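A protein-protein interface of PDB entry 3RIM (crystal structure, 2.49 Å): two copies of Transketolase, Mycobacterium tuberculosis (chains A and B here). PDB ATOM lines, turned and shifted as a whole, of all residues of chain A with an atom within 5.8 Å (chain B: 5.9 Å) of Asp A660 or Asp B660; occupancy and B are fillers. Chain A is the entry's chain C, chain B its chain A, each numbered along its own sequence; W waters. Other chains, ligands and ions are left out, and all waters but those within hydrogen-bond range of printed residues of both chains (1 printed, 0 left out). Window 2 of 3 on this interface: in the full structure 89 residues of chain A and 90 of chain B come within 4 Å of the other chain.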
ATOM      1  N   SER A 641      12.243 -20.921   7.100  1.00  0.00           N
ATOM      2  CA  SER A 641      11.031 -20.460   7.789  1.00  0.00           C
ATOM      3  C   SER A 641      10.689 -18.983   7.529  1.00  0.00           C
ATOM      4  O   SER A 641       9.556 -18.554   7.807  1.00  0.00           O
ATOM      5  CB  SER A 641      11.175 -20.593   9.305  1.00  0.00           C
ATOM      6  OG  SER A 641      11.300 -21.935   9.705  1.00  0.00           O
ATOM      7  N   HIS A 655      -1.963 -18.703   5.938  1.00  0.00           N
ATOM      8  CA  HIS A 655      -1.263 -19.057   7.157  1.00  0.00           C
ATOM      9  C   HIS A 655      -0.490 -20.379   7.105  1.00  0.00           C
ATOM     10  O   HIS A 655       0.657 -20.440   7.553  1.00  0.00           O
ATOM     11  CB  HIS A 655      -2.216 -19.027   8.354  1.00  0.00           C
ATOM     12  CG  HIS A 655      -2.730 -17.664   8.674  1.00  0.00           C
ATOM     13  ND1 HIS A 655      -1.937 -16.681   9.226  1.00  0.00           N
ATOM     14  CD2 HIS A 655      -3.955 -17.110   8.506  1.00  0.00           C
ATOM     15  CE1 HIS A 655      -2.658 -15.585   9.400  1.00  0.00           C
ATOM     16  NE2 HIS A 655      -3.889 -15.821   8.974  1.00  0.00           N
ATOM     17  N   GLN A 656      -1.111 -21.435   6.562  1.00  0.00           N
ATOM     18  CA  GLN A 656      -0.467 -22.729   6.473  1.00  0.00           C
ATOM     19  C   GLN A 656       0.822 -22.629   5.672  1.00  0.00           C
ATOM     20  O   GLN A 656       1.839 -23.252   6.001  1.00  0.00           O
ATOM     21  CB  GLN A 656      -1.384 -23.740   5.830  1.00  0.00           C
ATOM     22  CG  GLN A 656      -0.636 -24.939   5.240  1.00  0.00           C
ATOM     23  CD  GLN A 656      -1.553 -25.865   4.522  1.00  0.00           C
ATOM     24  OE1 GLN A 656      -2.534 -25.442   3.913  1.00  0.00           O
ATOM     25  NE2 GLN A 656      -1.261 -27.143   4.594  1.00  0.00           N
ATOM     26  N   VAL A 658       2.858 -19.840   5.199  1.00  0.00           N
ATOM     27  CA  VAL A 658       3.965 -19.043   5.772  1.00  0.00           C
ATOM     28  C   VAL A 658       4.367 -19.497   7.204  1.00  0.00           C
ATOM     29  O   VAL A 658       5.383 -19.063   7.753  1.00  0.00           O
ATOM     30  CB  VAL A 658       3.658 -17.505   5.740  1.00  0.00           C
ATOM     31  CG1 VAL A 658       3.144 -17.074   4.377  1.00  0.00           C
ATOM     32  CG2 VAL A 658       2.666 -17.115   6.841  1.00  0.00           C
ATOM     33  N   GLY A 659       3.548 -20.355   7.803  1.00  0.00           N
ATOM     34  CA  GLY A 659       3.841 -20.918   9.113  1.00  0.00           C
ATOM     35  C   GLY A 659       3.894 -19.903  10.239  1.00  0.00           C
ATOM     36  O   GLY A 659       3.678 -18.704  10.007  1.00  0.00           O
ATOM     37  N   ASP A 660       4.187 -20.417  11.448  1.00  0.00           N
ATOM     38  CA  ASP A 660       4.349 -19.676  12.746  1.00  0.00           C
ATOM     39  C   ASP A 660       5.105 -18.320  12.726  1.00  0.00           C
ATOM     40  O   ASP A 660       4.694 -17.344  13.382  1.00  0.00           O
ATOM     41  CB  ASP A 660       5.082 -20.600  13.763  1.00  0.00           C
ATOM     42  CG  ASP A 660       4.141 -21.287  14.789  1.00  0.00           C
ATOM     43  OD1 ASP A 660       3.139 -20.669  15.229  1.00  0.00           O
ATOM     44  OD2 ASP A 660       4.450 -22.438  15.199  1.00  0.00           O
ATOM     45  N   THR A 661       6.219 -18.287  11.999  1.00  0.00           N
ATOM     46  CA  THR A 661       7.144 -17.161  12.054  1.00  0.00           C
ATOM     47  C   THR A 661       7.138 -16.356  10.773  1.00  0.00           C
ATOM     48  O   THR A 661       8.049 -15.554  10.534  1.00  0.00           O
ATOM     49  CB  THR A 661       8.628 -17.611  12.365  1.00  0.00           C
ATOM     50  OG1 THR A 661       9.206 -18.278  11.226  1.00  0.00           O
ATOM     51  CG2 THR A 661       8.722 -18.496  13.663  1.00  0.00           C
ATOM     52  N   GLY A 662       6.117 -16.561   9.948  1.00  0.00           N
ATOM     53  CA  GLY A 662       5.989 -15.829   8.682  1.00  0.00           C
ATOM     54  C   GLY A 662       5.113 -14.608   8.848  1.00  0.00           C
ATOM     55  O   GLY A 662       4.500 -14.401   9.889  1.00  0.00           O
ATOM     56  N   SER B 641       2.778 -25.169  22.267  1.00  0.00           N
ATOM     57  CA  SER B 641       2.710 -25.287  20.814  1.00  0.00           C
ATOM     58  C   SER B 641       1.915 -26.511  20.352  1.00  0.00           C
ATOM     59  O   SER B 641       1.482 -26.582  19.192  1.00  0.00           O
ATOM     60  CB  SER B 641       4.106 -25.381  20.247  1.00  0.00           C
ATOM     61  OG  SER B 641       4.886 -24.288  20.701  1.00  0.00           O
ATOM     62  N   HIS B 655      -5.410 -22.926  10.643  1.00  0.00           N
ATOM     63  CA  HIS B 655      -3.950 -22.970  10.612  1.00  0.00           C
ATOM     64  C   HIS B 655      -3.264 -21.903  11.488  1.00  0.00           C
ATOM     65  O   HIS B 655      -2.257 -22.190  12.139  1.00  0.00           O
ATOM     66  CB  HIS B 655      -3.412 -22.895   9.165  1.00  0.00           C
ATOM     67  CG  HIS B 655      -3.797 -24.076   8.319  1.00  0.00           C
ATOM     68  ND1 HIS B 655      -3.195 -25.310   8.444  1.00  0.00           N
ATOM     69  CD2 HIS B 655      -4.731 -24.217   7.345  1.00  0.00           C
ATOM     70  CE1 HIS B 655      -3.737 -26.159   7.585  1.00  0.00           C
ATOM     71  NE2 HIS B 655      -4.665 -25.518   6.899  1.00  0.00           N
ATOM     72  N   GLN B 656      -3.785 -20.681  11.505  1.00  0.00           N
ATOM     73  CA  GLN B 656      -3.115 -19.601  12.239  1.00  0.00           C
ATOM     74  C   GLN B 656      -3.146 -19.919  13.727  1.00  0.00           C
ATOM     75  O   GLN B 656      -2.180 -19.662  14.440  1.00  0.00           O
ATOM     76  CB  GLN B 656      -3.792 -18.275  11.974  1.00  0.00           C
ATOM     77  CG  GLN B 656      -3.542 -17.235  13.040  1.00  0.00           C
ATOM     78  CD  GLN B 656      -4.290 -15.938  12.755  1.00  0.00           C
ATOM     79  OE1 GLN B 656      -5.465 -15.932  12.327  1.00  0.00           O
ATOM     80  NE2 GLN B 656      -3.609 -14.830  12.991  1.00  0.00           N
ATOM     81  N   VAL B 658      -3.430 -23.106  15.196  1.00  0.00           N
ATOM     82  CA  VAL B 658      -2.677 -24.298  15.648  1.00  0.00           C
ATOM     83  C   VAL B 658      -1.160 -24.214  15.409  1.00  0.00           C
ATOM     84  O   VAL B 658      -0.391 -24.983  15.989  1.00  0.00           O
ATOM     85  CB  VAL B 658      -3.240 -25.654  15.102  1.00  0.00           C
ATOM     86  CG1 VAL B 658      -4.724 -25.752  15.326  1.00  0.00           C
ATOM     87  CG2 VAL B 658      -2.869 -25.856  13.635  1.00  0.00           C
ATOM     88  N   GLY B 659      -0.738 -23.296  14.549  1.00  0.00           N
ATOM     89  CA  GLY B 659       0.679 -23.052  14.312  1.00  0.00           C
ATOM     90  C   GLY B 659       1.361 -24.171  13.549  1.00  0.00           C
ATOM     91  O   GLY B 659       0.719 -25.171  13.210  1.00  0.00           O
ATOM     92  N   ASP B 660       2.667 -23.980  13.306  1.00  0.00           N
ATOM     93  CA  ASP B 660       3.601 -24.910  12.592  1.00  0.00           C
ATOM     94  C   ASP B 660       3.537 -26.385  12.959  1.00  0.00           C
ATOM     95  O   ASP B 660       3.617 -27.279  12.080  1.00  0.00           O
ATOM     96  CB  ASP B 660       5.063 -24.477  12.830  1.00  0.00           C
ATOM     97  CG  ASP B 660       5.636 -23.648  11.687  1.00  0.00           C
ATOM     98  OD1 ASP B 660       5.226 -23.838  10.510  1.00  0.00           O
ATOM     99  OD2 ASP B 660       6.526 -22.812  11.977  1.00  0.00           O
ATOM    100  N   THR B 661       3.433 -26.620  14.266  1.00  0.00           N
ATOM    101  CA  THR B 661       3.526 -27.960  14.817  1.00  0.00           C
ATOM    102  C   THR B 661       2.206 -28.522  15.269  1.00  0.00           C
ATOM    103  O   THR B 661       2.189 -29.541  15.922  1.00  0.00           O
ATOM    104  CB  THR B 661       4.560 -28.024  15.970  1.00  0.00           C
ATOM    105  OG1 THR B 661       4.084 -27.287  17.115  1.00  0.00           O
ATOM    106  CG2 THR B 661       5.918 -27.457  15.479  1.00  0.00           C
ATOM    107  N   GLY B 662       1.108 -27.873  14.888  1.00  0.00           N
ATOM    108  CA  GLY B 662      -0.228 -28.287  15.307  1.00  0.00           C
ATOM    109  C   GLY B 662      -0.816 -29.256  14.327  1.00  0.00           C
ATOM    110  O   GLY B 662      -0.258 -29.477  13.251  1.00  0.00           O
HETATM  111  O   HOH W   1      -5.050 -23.425   4.311  1.00  0.00           O
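Among the printed residues, merely in contact across the chains: His A655 with Gln B656, Gln A656 with His B655, Gly A659 with Asp B660 and Asp A660 with Gly B659.
His A655 touches Gln B656, and with the chains exchanged Gln A656 touches His B655. Gly A659 touches Asp B660, and with the chains exchanged Asp A660 touches Gly B659. Asp B660 touches its own counterpart, Asp A660. Positions printed for both chains: 641, 655, 656, 658, 659, 660, 661 and 662. Of the 5 pairs that touch across the chains among the printed residues, 5 have their exchanged pair printed and touching as well.
Of the printed residues of chain B, His A655 touches Gln B656 (3.5 Å). Printed residues of chain B within 4 Å of Gln A656: His B655 (3.5 Å). Asp A660 touches just these residues of chain B: Gly B659 and Asp B660. Ser B641 touches none of the printed residues of chain A. Printed residues of chain A within 4 Å of His B655: Gln A656 (3.5 Å). Of the printed residues of chain A, Gly B659 touches Asp A660. The nearest residue of chain B that does not touch Asp A660 is Thr B661 (4.4 Å). The nearest printed residue of chain A that does not touch Gln B656 is Asp A660 (5.5 Å).
Water W1 bridges the side-chain amide oxygen of Gln A656 and a ring nitrogen (NE2) of His B655.
The backbone NH (N) of Asp B660 sits at hydrogen-bond distance from the side-chain carboxylate (OD2) of Asp A660, 3.0 Å away.
Printed residues of chain A that touch a printed residue of chain B: His A655, Gln A656, Gly A659 and Asp A660. Hydrophobic or aromatic side chains of chain A that line the printed part of chain B: His A655. Of the 8 printed residues of chain B, 4 touch a printed residue of chain A. Hydrophobic or aromatic side chains of chain B within 4 Å of the printed part of chain A: His B655.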
